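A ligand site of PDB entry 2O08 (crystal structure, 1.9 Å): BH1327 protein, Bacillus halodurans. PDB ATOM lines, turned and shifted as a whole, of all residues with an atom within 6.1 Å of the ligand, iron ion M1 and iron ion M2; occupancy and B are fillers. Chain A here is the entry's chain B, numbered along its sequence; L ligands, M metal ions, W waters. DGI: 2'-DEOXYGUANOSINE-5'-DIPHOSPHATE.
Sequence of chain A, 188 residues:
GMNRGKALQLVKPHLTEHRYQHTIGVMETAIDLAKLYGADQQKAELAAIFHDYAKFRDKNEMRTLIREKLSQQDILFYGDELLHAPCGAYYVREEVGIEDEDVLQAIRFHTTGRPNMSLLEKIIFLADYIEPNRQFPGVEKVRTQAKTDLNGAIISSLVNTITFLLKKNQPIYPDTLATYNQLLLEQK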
ATOM      1  N   ARG A  19      28.703  20.182  19.212  1.00  0.00           N
ATOM      2  CA  ARG A  19      28.008  18.937  18.904  1.00  0.00           C
ATOM      3  C   ARG A  19      28.459  17.747  19.774  1.00  0.00           C
ATOM      4  O   ARG A  19      27.631  16.866  20.100  1.00  0.00           O
ATOM      5  CB  ARG A  19      28.239  18.652  17.426  1.00  0.00           C
ATOM      6  CG  ARG A  19      27.422  17.546  16.855  1.00  0.00           C
ATOM      7  CD  ARG A  19      25.953  17.732  16.949  1.00  0.00           C
ATOM      8  NE  ARG A  19      25.483  19.114  16.834  1.00  0.00           N
ATOM      9  CZ  ARG A  19      24.285  19.440  16.373  1.00  0.00           C
ATOM     10  NH1 ARG A  19      23.461  18.509  15.968  1.00  0.00           N
ATOM     11  NH2 ARG A  19      23.924  20.721  16.297  1.00  0.00           N
ATOM     12  N   HIS A  22      26.629  18.243  22.891  1.00  0.00           N
ATOM     13  CA  HIS A  22      25.257  17.813  22.621  1.00  0.00           C
ATOM     14  C   HIS A  22      25.168  16.320  22.794  1.00  0.00           C
ATOM     15  O   HIS A  22      24.255  15.823  23.447  1.00  0.00           O
ATOM     16  CB  HIS A  22      24.838  18.241  21.200  1.00  0.00           C
ATOM     17  CG  HIS A  22      23.663  17.496  20.634  1.00  0.00           C
ATOM     18  ND1 HIS A  22      22.383  17.695  21.076  1.00  0.00           N
ATOM     19  CD2 HIS A  22      23.577  16.596  19.615  1.00  0.00           C
ATOM     20  CE1 HIS A  22      21.561  16.946  20.376  1.00  0.00           C
ATOM     21  NE2 HIS A  22      22.255  16.269  19.477  1.00  0.00           N
ATOM     22  N   THR A  23      26.130  15.608  22.207  1.00  0.00           N
ATOM     23  CA  THR A  23      26.171  14.126  22.232  1.00  0.00           C
ATOM     24  C   THR A  23      26.250  13.567  23.654  1.00  0.00           C
ATOM     25  O   THR A  23      25.527  12.626  23.990  1.00  0.00           O
ATOM     26  CB  THR A  23      27.288  13.618  21.329  1.00  0.00           C
ATOM     27  OG1 THR A  23      27.016  14.038  19.973  1.00  0.00           O
ATOM     28  CG2 THR A  23      27.373  12.096  21.372  1.00  0.00           C
ATOM     29  N   VAL A  26      22.845  13.987  25.072  1.00  0.00           N
ATOM     30  CA  VAL A  26      21.909  12.990  24.563  1.00  0.00           C
ATOM     31  C   VAL A  26      22.174  11.651  25.267  1.00  0.00           C
ATOM     32  O   VAL A  26      21.216  10.951  25.685  1.00  0.00           O
ATOM     33  CB  VAL A  26      21.975  12.821  23.005  1.00  0.00           C
ATOM     34  CG1 VAL A  26      20.997  11.738  22.563  1.00  0.00           C
ATOM     35  CG2 VAL A  26      21.662  14.143  22.318  1.00  0.00           C
ATOM     36  N   HIS A  51      24.768   8.886  17.373  1.00  0.00           N
ATOM     37  CA  HIS A  51      23.592   9.339  16.613  1.00  0.00           C
ATOM     38  C   HIS A  51      23.924  10.407  15.573  1.00  0.00           C
ATOM     39  O   HIS A  51      23.450  10.289  14.444  1.00  0.00           O
ATOM     40  CB  HIS A  51      22.401   9.761  17.528  1.00  0.00           C
ATOM     41  CG  HIS A  51      22.494  11.143  18.056  1.00  0.00           C
ATOM     42  ND1 HIS A  51      23.381  11.524  19.039  1.00  0.00           N
ATOM     43  CD2 HIS A  51      21.817  12.266  17.714  1.00  0.00           C
ATOM     44  CE1 HIS A  51      23.266  12.823  19.265  1.00  0.00           C
ATOM     45  NE2 HIS A  51      22.304  13.293  18.493  1.00  0.00           N
ATOM     46  N   ASP A  52      24.809  11.350  15.918  1.00  0.00           N
ATOM     47  CA  ASP A  52      25.289  12.443  15.024  1.00  0.00           C
ATOM     48  C   ASP A  52      26.647  12.231  14.380  1.00  0.00           C
ATOM     49  O   ASP A  52      27.299  13.188  13.932  1.00  0.00           O
ATOM     50  CB  ASP A  52      25.241  13.776  15.789  1.00  0.00           C
ATOM     51  CG  ASP A  52      23.832  14.357  15.843  1.00  0.00           C
ATOM     52  OD1 ASP A  52      23.004  13.918  15.004  1.00  0.00           O
ATOM     53  OD2 ASP A  52      23.571  15.273  16.671  1.00  0.00           O
ATOM     54  N   LYS A  55      26.783  13.848  11.118  1.00  0.00           N
ATOM     55  CA  LYS A  55      26.250  15.199  11.031  1.00  0.00           C
ATOM     56  C   LYS A  55      27.034  16.126  10.073  1.00  0.00           C
ATOM     57  O   LYS A  55      26.428  16.967   9.369  1.00  0.00           O
ATOM     58  CB  LYS A  55      26.173  15.812  12.428  1.00  0.00           C
ATOM     59  CG  LYS A  55      25.586  17.193  12.522  1.00  0.00           C
ATOM     60  CD  LYS A  55      24.117  17.190  12.425  1.00  0.00           C
ATOM     61  CE  LYS A  55      23.576  18.602  12.507  1.00  0.00           C
ATOM     62  NZ  LYS A  55      22.110  18.572  12.314  1.00  0.00           N
ATOM     63  N   TYR A  78      13.413  16.262   0.839  1.00  0.00           N
ATOM     64  CA  TYR A  78      12.896  16.960   2.012  1.00  0.00           C
ATOM     65  C   TYR A  78      13.890  17.576   2.954  1.00  0.00           C
ATOM     66  O   TYR A  78      13.562  17.729   4.108  1.00  0.00           O
ATOM     67  CB  TYR A  78      11.990  16.027   2.803  1.00  0.00           C
ATOM     68  CG  TYR A  78      10.805  15.552   2.034  1.00  0.00           C
ATOM     69  CD1 TYR A  78       9.673  16.327   1.906  1.00  0.00           C
ATOM     70  CD2 TYR A  78      10.834  14.322   1.402  1.00  0.00           C
ATOM     71  CE1 TYR A  78       8.570  15.872   1.189  1.00  0.00           C
ATOM     72  CE2 TYR A  78       9.751  13.876   0.666  1.00  0.00           C
ATOM     73  CZ  TYR A  78       8.612  14.652   0.575  1.00  0.00           C
ATOM     74  OH  TYR A  78       7.536  14.175  -0.133  1.00  0.00           O
ATOM     75  N   GLY A  79      15.076  17.938   2.510  1.00  0.00           N
ATOM     76  CA  GLY A  79      16.007  18.682   3.344  1.00  0.00           C
ATOM     77  C   GLY A  79      17.323  17.958   3.616  1.00  0.00           C
ATOM     78  O   GLY A  79      17.344  16.750   3.933  1.00  0.00           O
ATOM     79  N   GLU A  81      19.183  18.105   6.134  1.00  0.00           N
ATOM     80  CA  GLU A  81      19.357  17.598   7.498  1.00  0.00           C
ATOM     81  C   GLU A  81      18.881  16.152   7.689  1.00  0.00           C
ATOM     82  O   GLU A  81      19.200  15.524   8.699  1.00  0.00           O
ATOM     83  CB  GLU A  81      18.717  18.527   8.533  1.00  0.00           C
ATOM     84  CG  GLU A  81      19.509  19.874   8.764  1.00  0.00           C
ATOM     85  CD  GLU A  81      21.010  19.670   9.041  1.00  0.00           C
ATOM     86  OE1 GLU A  81      21.371  18.715   9.768  1.00  0.00           O
ATOM     87  OE2 GLU A  81      21.827  20.467   8.515  1.00  0.00           O
ATOM     88  N   LEU A  82      18.145  15.628   6.706  1.00  0.00           N
ATOM     89  CA  LEU A  82      17.625  14.286   6.778  1.00  0.00           C
ATOM     90  C   LEU A  82      18.638  13.228   6.363  1.00  0.00           C
ATOM     91  O   LEU A  82      18.381  12.019   6.471  1.00  0.00           O
ATOM     92  CB  LEU A  82      16.380  14.170   5.909  1.00  0.00           C
ATOM     93  CG  LEU A  82      15.199  15.096   6.248  1.00  0.00           C
ATOM     94  CD1 LEU A  82      13.907  14.450   5.710  1.00  0.00           C
ATOM     95  CD2 LEU A  82      15.112  15.272   7.712  1.00  0.00           C
ATOM     96  N   HIS A  84      21.934  12.736   7.527  1.00  0.00           N
ATOM     97  CA  HIS A  84      22.892  12.239   8.488  1.00  0.00           C
ATOM     98  C   HIS A  84      22.458  11.063   9.329  1.00  0.00           C
ATOM     99  O   HIS A  84      23.313  10.219   9.627  1.00  0.00           O
ATOM    100  CB  HIS A  84      23.454  13.385   9.334  1.00  0.00           C
ATOM    101  CG  HIS A  84      22.522  13.915  10.401  1.00  0.00           C
ATOM    102  ND1 HIS A  84      21.616  14.925  10.153  1.00  0.00           N
ATOM    103  CD2 HIS A  84      22.469  13.682  11.731  1.00  0.00           C
ATOM    104  CE1 HIS A  84      20.968  15.215  11.276  1.00  0.00           C
ATOM    105  NE2 HIS A  84      21.468  14.476  12.246  1.00  0.00           N
ATOM    106  N   ALA A  85      21.176  11.002   9.697  1.00  0.00           N
ATOM    107  CA  ALA A  85      20.657   9.863  10.474  1.00  0.00           C
ATOM    108  C   ALA A  85      20.799   8.512   9.725  1.00  0.00           C
ATOM    109  O   ALA A  85      21.496   7.602  10.215  1.00  0.00           O
ATOM    110  CB  ALA A  85      19.168  10.099  10.968  1.00  0.00           C
ATOM    111  N   HIS A 110      16.483   8.875  14.226  1.00  0.00           N
ATOM    112  CA  HIS A 110      16.515   9.904  15.288  1.00  0.00           C
ATOM    113  C   HIS A 110      16.114  11.303  14.812  1.00  0.00           C
ATOM    114  O   HIS A 110      15.746  12.146  15.646  1.00  0.00           O
ATOM    115  CB  HIS A 110      17.895   9.994  15.966  1.00  0.00           C
ATOM    116  CG  HIS A 110      18.890  10.835  15.250  1.00  0.00           C
ATOM    117  ND1 HIS A 110      19.862  10.304  14.420  1.00  0.00           N
ATOM    118  CD2 HIS A 110      19.132  12.173  15.291  1.00  0.00           C
ATOM    119  CE1 HIS A 110      20.625  11.280  13.949  1.00  0.00           C
ATOM    120  NE2 HIS A 110      20.197  12.422  14.463  1.00  0.00           N
ATOM    121  N   THR A 111      16.214  11.550  13.496  1.00  0.00           N
ATOM    122  CA  THR A 111      15.889  12.862  12.921  1.00  0.00           C
ATOM    123  C   THR A 111      14.374  12.897  12.544  1.00  0.00           C
ATOM    124  O   THR A 111      13.687  13.752  13.054  1.00  0.00           O
ATOM    125  CB  THR A 111      16.782  13.263  11.708  1.00  0.00           C
ATOM    126  OG1 THR A 111      18.153  13.288  12.131  1.00  0.00           O
ATOM    127  CG2 THR A 111      16.395  14.690  11.151  1.00  0.00           C
ATOM    128  N   THR A 112      13.879  11.950  11.749  1.00  0.00           N
ATOM    129  CA  THR A 112      12.499  12.017  11.270  1.00  0.00           C
ATOM    130  C   THR A 112      11.480  11.335  12.150  1.00  0.00           C
ATOM    131  O   THR A 112      10.320  11.701  12.113  1.00  0.00           O
ATOM    132  CB  THR A 112      12.340  11.390   9.895  1.00  0.00           C
ATOM    133  OG1 THR A 112      12.767  10.002   9.951  1.00  0.00           O
ATOM    134  CG2 THR A 112      13.133  12.161   8.890  1.00  0.00           C
ATOM    135  N   ASP A 128      17.463  13.401  22.074  1.00  0.00           N
ATOM    136  CA  ASP A 128      18.053  14.367  21.123  1.00  0.00           C
ATOM    137  C   ASP A 128      17.396  15.720  21.282  1.00  0.00           C
ATOM    138  O   ASP A 128      18.043  16.743  21.236  1.00  0.00           O
ATOM    139  CB  ASP A 128      17.863  13.886  19.683  1.00  0.00           C
ATOM    140  CG  ASP A 128      18.665  14.707  18.666  1.00  0.00           C
ATOM    141  OD1 ASP A 128      19.777  15.118  18.984  1.00  0.00           O
ATOM    142  OD2 ASP A 128      18.200  14.927  17.535  1.00  0.00           O
ATOM    143  N   ARG A 134      19.984  21.981  24.994  1.00  0.00           N
ATOM    144  CA  ARG A 134      19.046  22.535  24.026  1.00  0.00           C
ATOM    145  C   ARG A 134      18.330  23.745  24.608  1.00  0.00           C
ATOM    146  O   ARG A 134      17.996  23.760  25.792  1.00  0.00           O
ATOM    147  CB  ARG A 134      18.003  21.512  23.607  1.00  0.00           C
ATOM    148  CG  ARG A 134      18.554  20.350  22.858  1.00  0.00           C
ATOM    149  CD  ARG A 134      19.040  20.710  21.474  1.00  0.00           C
ATOM    150  NE  ARG A 134      18.791  19.577  20.568  1.00  0.00           N
ATOM    151  CZ  ARG A 134      19.409  19.338  19.415  1.00  0.00           C
ATOM    152  NH1 ARG A 134      20.387  20.111  18.964  1.00  0.00           N
ATOM    153  NH2 ARG A 134      19.061  18.273  18.702  1.00  0.00           N
ATOM    154  N   THR A 161       8.798  20.990  16.191  1.00  0.00           N
ATOM    155  CA  THR A 161       9.613  20.801  14.990  1.00  0.00           C
ATOM    156  C   THR A 161       8.836  21.124  13.712  1.00  0.00           C
ATOM    157  O   THR A 161       9.267  21.943  12.904  1.00  0.00           O
ATOM    158  CB  THR A 161      10.167  19.350  14.959  1.00  0.00           C
ATOM    159  OG1 THR A 161      11.004  19.150  16.117  1.00  0.00           O
ATOM    160  CG2 THR A 161      10.936  19.036  13.674  1.00  0.00           C
ATOM    161  N   ILE A 162       7.659  20.515  13.561  1.00  0.00           N
ATOM    162  CA  ILE A 162       6.868  20.714  12.354  1.00  0.00           C
ATOM    163  C   ILE A 162       6.451  22.187  12.249  1.00  0.00           C
ATOM    164  O   ILE A 162       6.510  22.781  11.161  1.00  0.00           O
ATOM    165  CB  ILE A 162       5.664  19.745  12.262  1.00  0.00           C
ATOM    166  CG1 ILE A 162       6.166  18.286  12.237  1.00  0.00           C
ATOM    167  CG2 ILE A 162       4.876  20.031  10.956  1.00  0.00           C
ATOM    168  CD1 ILE A 162       5.060  17.210  12.354  1.00  0.00           C
ATOM    169  N   PHE A 164       8.065  24.776  13.387  1.00  0.00           N
ATOM    170  CA  PHE A 164       9.257  25.518  12.998  1.00  0.00           C
ATOM    171  C   PHE A 164       9.502  25.405  11.503  1.00  0.00           C
ATOM    172  O   PHE A 164       9.701  26.422  10.839  1.00  0.00           O
ATOM    173  CB  PHE A 164      10.433  25.000  13.816  1.00  0.00           C
ATOM    174  CG  PHE A 164      11.728  25.630  13.454  1.00  0.00           C
ATOM    175  CD1 PHE A 164      12.122  26.805  14.059  1.00  0.00           C
ATOM    176  CD2 PHE A 164      12.537  25.074  12.451  1.00  0.00           C
ATOM    177  CE1 PHE A 164      13.336  27.399  13.714  1.00  0.00           C
ATOM    178  CE2 PHE A 164      13.734  25.682  12.084  1.00  0.00           C
ATOM    179  CZ  PHE A 164      14.129  26.827  12.709  1.00  0.00           C
ATOM    180  N   LEU A 165       9.467  24.174  10.966  1.00  0.00           N
ATOM    181  CA  LEU A 165       9.653  23.975   9.511  1.00  0.00           C
ATOM    182  C   LEU A 165       8.625  24.759   8.677  1.00  0.00           C
ATOM    183  O   LEU A 165       8.971  25.438   7.706  1.00  0.00           O
ATOM    184  CB  LEU A 165       9.626  22.452   9.174  1.00  0.00           C
ATOM    185  CG  LEU A 165      10.782  21.593   9.754  1.00  0.00           C
ATOM    186  CD1 LEU A 165      10.490  20.044   9.773  1.00  0.00           C
ATOM    187  CD2 LEU A 165      12.114  21.951   8.967  1.00  0.00           C
ATOM    188  N   GLN A 170       9.946  25.381   4.952  1.00  0.00           N
ATOM    189  CA  GLN A 170      10.839  24.286   4.566  1.00  0.00           C
ATOM    190  C   GLN A 170       9.937  23.036   4.369  1.00  0.00           C
ATOM    191  O   GLN A 170       8.850  22.969   4.942  1.00  0.00           O
ATOM    192  CB  GLN A 170      11.919  24.115   5.639  1.00  0.00           C
ATOM    193  CG  GLN A 170      12.954  25.287   5.663  1.00  0.00           C
ATOM    194  CD  GLN A 170      13.921  25.267   6.876  1.00  0.00           C
ATOM    195  OE1 GLN A 170      13.837  24.385   7.746  1.00  0.00           O
ATOM    196  NE2 GLN A 170      14.847  26.233   6.920  1.00  0.00           N
ATOM    197  N   PRO A 171      10.353  22.097   3.522  1.00  0.00           N
ATOM    198  CA  PRO A 171       9.557  20.903   3.345  1.00  0.00           C
ATOM    199  C   PRO A 171       9.559  20.046   4.585  1.00  0.00           C
ATOM    200  O   PRO A 171      10.430  20.190   5.425  1.00  0.00           O
ATOM    201  CB  PRO A 171      10.238  20.201   2.161  1.00  0.00           C
ATOM    202  CG  PRO A 171      11.642  20.649   2.257  1.00  0.00           C
ATOM    203  CD  PRO A 171      11.552  22.077   2.664  1.00  0.00           C
ATOM    204  N   ILE A 172       8.516  19.242   4.759  1.00  0.00           N
ATOM    205  CA  ILE A 172       8.357  18.413   5.939  1.00  0.00           C
ATOM    206  C   ILE A 172       8.219  16.954   5.470  1.00  0.00           C
ATOM    207  O   ILE A 172       7.293  16.603   4.739  1.00  0.00           O
ATOM    208  CB  ILE A 172       7.119  18.884   6.740  1.00  0.00           C
ATOM    209  CG1 ILE A 172       7.358  20.338   7.206  1.00  0.00           C
ATOM    210  CG2 ILE A 172       6.852  17.947   7.918  1.00  0.00           C
ATOM    211  CD1 ILE A 172       6.115  21.090   7.554  1.00  0.00           C
ATOM    212  N   TYR A 173       9.138  16.112   5.891  1.00  0.00           N
ATOM    213  CA  TYR A 173       9.153  14.708   5.524  1.00  0.00           C
ATOM    214  C   TYR A 173       7.818  14.075   5.926  1.00  0.00           C
ATOM    215  O   TYR A 173       7.411  14.198   7.080  1.00  0.00           O
ATOM    216  CB  TYR A 173      10.265  13.981   6.255  1.00  0.00           C
ATOM    217  CG  TYR A 173      10.510  12.581   5.767  1.00  0.00           C
ATOM    218  CD1 TYR A 173      10.842  12.341   4.428  1.00  0.00           C
ATOM    219  CD2 TYR A 173      10.511  11.520   6.636  1.00  0.00           C
ATOM    220  CE1 TYR A 173      11.115  11.077   3.986  1.00  0.00           C
ATOM    221  CE2 TYR A 173      10.800  10.240   6.204  1.00  0.00           C
ATOM    222  CZ  TYR A 173      11.090  10.026   4.886  1.00  0.00           C
ATOM    223  OH  TYR A 173      11.353   8.758   4.454  1.00  0.00           O
ATOM    224  N   PRO A 174       7.124  13.447   4.975  1.00  0.00           N
ATOM    225  CA  PRO A 174       5.817  12.904   5.297  1.00  0.00           C
ATOM    226  C   PRO A 174       5.742  11.892   6.420  1.00  0.00           C
ATOM    227  O   PRO A 174       4.753  11.878   7.152  1.00  0.00           O
ATOM    228  CB  PRO A 174       5.362  12.298   3.973  1.00  0.00           C
ATOM    229  CG  PRO A 174       6.129  12.984   2.945  1.00  0.00           C
ATOM    230  CD  PRO A 174       7.435  13.293   3.533  1.00  0.00           C
ATOM    231  N   THR A 176       7.381  11.960   9.133  1.00  0.00           N
ATOM    232  CA  THR A 176       7.386  12.691  10.400  1.00  0.00           C
ATOM    233  C   THR A 176       5.959  13.071  10.820  1.00  0.00           C
ATOM    234  O   THR A 176       5.615  12.985  11.991  1.00  0.00           O
ATOM    235  CB  THR A 176       8.273  13.914  10.342  1.00  0.00           C
ATOM    236  OG1 THR A 176       9.616  13.474  10.098  1.00  0.00           O
ATOM    237  CG2 THR A 176       8.212  14.720  11.681  1.00  0.00           C
ATOM    238  N   LEU A 177       5.147  13.528   9.888  1.00  0.00           N
ATOM    239  CA  LEU A 177       3.745  13.768  10.218  1.00  0.00           C
ATOM    240  C   LEU A 177       3.073  12.402  10.516  1.00  0.00           C
ATOM    241  O   LEU A 177       2.277  12.346  11.447  1.00  0.00           O
ATOM    242  CB  LEU A 177       3.030  14.568   9.121  1.00  0.00           C
ATOM    243  CG  LEU A 177       1.583  14.987   9.439  1.00  0.00           C
ATOM    244  CD1 LEU A 177       1.570  16.099  10.510  1.00  0.00           C
ATOM    245  CD2 LEU A 177       0.792  15.411   8.170  1.00  0.00           C
HETATM  246  O1B DGI L   1      21.349  16.611  14.403  1.00  0.00           O
HETATM  247  PB  DGI L   1      20.739  17.616  15.352  1.00  0.00           P
HETATM  248  O2B DGI L   1      21.244  17.362  16.770  1.00  0.00           O
HETATM  249  O3B DGI L   1      20.587  19.024  14.854  1.00  0.00           O
HETATM  250  O3A DGI L   1      19.180  17.158  15.444  1.00  0.00           O
HETATM  251  PA  DGI L   1      18.285  16.491  14.240  1.00  0.00           P
HETATM  252  O1A DGI L   1      18.870  15.189  13.714  1.00  0.00           O
HETATM  253  O2A DGI L   1      16.897  16.291  14.832  1.00  0.00           O
HETATM  254  O5' DGI L   1      18.326  17.641  13.055  1.00  0.00           O
HETATM  255  C5' DGI L   1      17.735  18.933  13.278  1.00  0.00           C
HETATM  256  C4' DGI L   1      17.205  19.502  11.963  1.00  0.00           C
HETATM  257  O4' DGI L   1      16.383  18.513  11.352  1.00  0.00           O
HETATM  258  C3' DGI L   1      16.367  20.777  12.013  1.00  0.00           C
HETATM  259  O3' DGI L   1      16.939  21.799  11.197  1.00  0.00           O
HETATM  260  C2' DGI L   1      15.016  20.424  11.433  1.00  0.00           C
HETATM  261  C1' DGI L   1      15.310  19.144  10.673  1.00  0.00           C
HETATM  262  N9  DGI L   1      14.193  18.190  10.669  1.00  0.00           N
HETATM  263  C8  DGI L   1      13.774  17.395  11.674  1.00  0.00           C
HETATM  264  N7  DGI L   1      12.704  16.636  11.289  1.00  0.00           N
HETATM  265  C5  DGI L   1      12.440  16.960  10.018  1.00  0.00           C
HETATM  266  C4  DGI L   1      13.426  17.988   9.634  1.00  0.00           C
HETATM  267  N3  DGI L   1      13.422  18.537   8.395  1.00  0.00           N
HETATM  268  C2  DGI L   1      12.475  18.129   7.498  1.00  0.00           C
HETATM  269  N2  DGI L   1      12.490  18.683   6.270  1.00  0.00           N
HETATM  270  N1  DGI L   1      11.514  17.201   7.791  1.00  0.00           N
HETATM  271  C6  DGI L   1      11.445  16.585   8.988  1.00  0.00           C
HETATM  272  O6  DGI L   1      10.581  15.742   9.216  1.00  0.00           O
HETATM  273 FE    FE M   1      20.955  14.582  14.369  1.00  0.00          FE
HETATM  274 FE    FE M   2      21.604  15.239  17.757  1.00  0.00          FE
HETATM  275  O   HOH W   1      20.450  14.690  16.221  1.00  0.00           O
HETATM  276  O   HOH W   2      15.012  20.525   7.191  1.00  0.00           O
HETATM  277  O   HOH W   3      14.023  15.870  14.705  1.00  0.00           O
HETATM  278  O   HOH W   4      17.873  20.963  15.640  1.00  0.00           O
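Water W1 lies within hydrogen-bond range of OD2 of Asp 128 and O3A of the ligand. Water W3 bridges O of Thr 111 (2.7 Å) and O2A of the ligand (2.9 Å).
OG1 of Thr 111 sits close to O1A of the ligand. N2 of the ligand lies within hydrogen-bond range of O of Tyr 78, 2.6 Å away. OG1 of Thr 176 lies within hydrogen-bond range of O6 of the ligand, at 2.6 Å. The guanidinium group of Arg 19 is in salt-bridge range of an oxygen (O3B) of the ligand, 3.1 Å away. The backbone carbonyl oxygen (O) of Pro 171 sits at hydrogen-bond distance from a nitrogen (N2) of the ligand (2.7 Å). The side-chain amino group of Lys 55 is in salt-bridge range of an oxygen (O3B) of the ligand (3.0 Å). The guanidinium group (NH2) of Arg 134 sits at hydrogen-bond distance from an oxygen (O3A) of the ligand, at 3.4 Å.
The backbone NH of Tyr 173 sits close to a nitrogen (N1) of the ligand (3.2 Å). Residues that only touch the ligand: Glu 81 (3.7 Å), Leu 82 (3.7 Å), Thr 161 (3.8 Å), Leu 165 (3.6 Å) and Ile 172 (3.9 Å). Hydrophobic or aromatic side chains within 4 Å of the ligand: His 22, Leu 82, His 84, His 110, Leu 165 and Tyr 173. The nearest printed residue that does not touch the ligand is Thr 112 (4.4 Å).
A ring nitrogen (ND1) of His 84 is in hydrogen-bond range of the backbone carbonyl oxygen (O) of Glu 81, at 2.9 Å. NH2 of Arg 134 is in salt-bridge range of OD2 of Asp 128 (3.6 Å). The guanidinium group of Arg 19 sits close to the side-chain carboxylate of Asp 52. OG1 of Thr 111 lies close to NE2 of His 110 (3.2 Å). The side-chain hydroxyl of Thr 176 sits at hydrogen-bond distance from the backbone carbonyl oxygen of Thr 112 (2.8 Å). The backbone carbonyl oxygen of Arg 19 is in hydrogen-bond range of the side-chain hydroxyl of Thr 23, at 2.9 Å. NZ of Lys 55 lies within salt-bridge range of OE1 of Glu 81, at 2.7 Å. N of Gln 170 sits at hydrogen-bond distance from O of Leu 165.
Water W1 binds iron ion M1, at 1.9 Å. Iron ion M1 is bound by O1B of the ligand (2.1 Å). Iron ion M1 is bound by a ring nitrogen (NE2) of His 84 (2.2 Å). OD1 of Asp 52 binds iron ion M1 (2.2 Å). O1A of the ligand is bound to iron ion M1, at 2.3 Å. NE2 of His 110 is bound to iron ion M1, 2.3 Å away. Iron ion M1 has six donor atoms within binding distance.
Of the 29 residues printed, 4 come within 4 Å of iron ion M2. The nearest printed residue that does not touch iron ion M2 is Arg 134 (4.1 Å).
Iron ion M2 is bound by water W1, a ring nitrogen (NE2) of His 22, a ring nitrogen (NE2) of His 51, the side-chain carboxylate of Asp 128, the side-chain carboxylate of Asp 52 and an oxygen (O2B) of the ligand.
Merely in contact with iron ion M1: Thr 111 (3.8 Å). Within 4 Å of iron ion M1: Asp 52, His 84, His 110 and Thr 111. The nearest printed residue that does not touch iron ion M1 is His 51 (4.2 Å).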
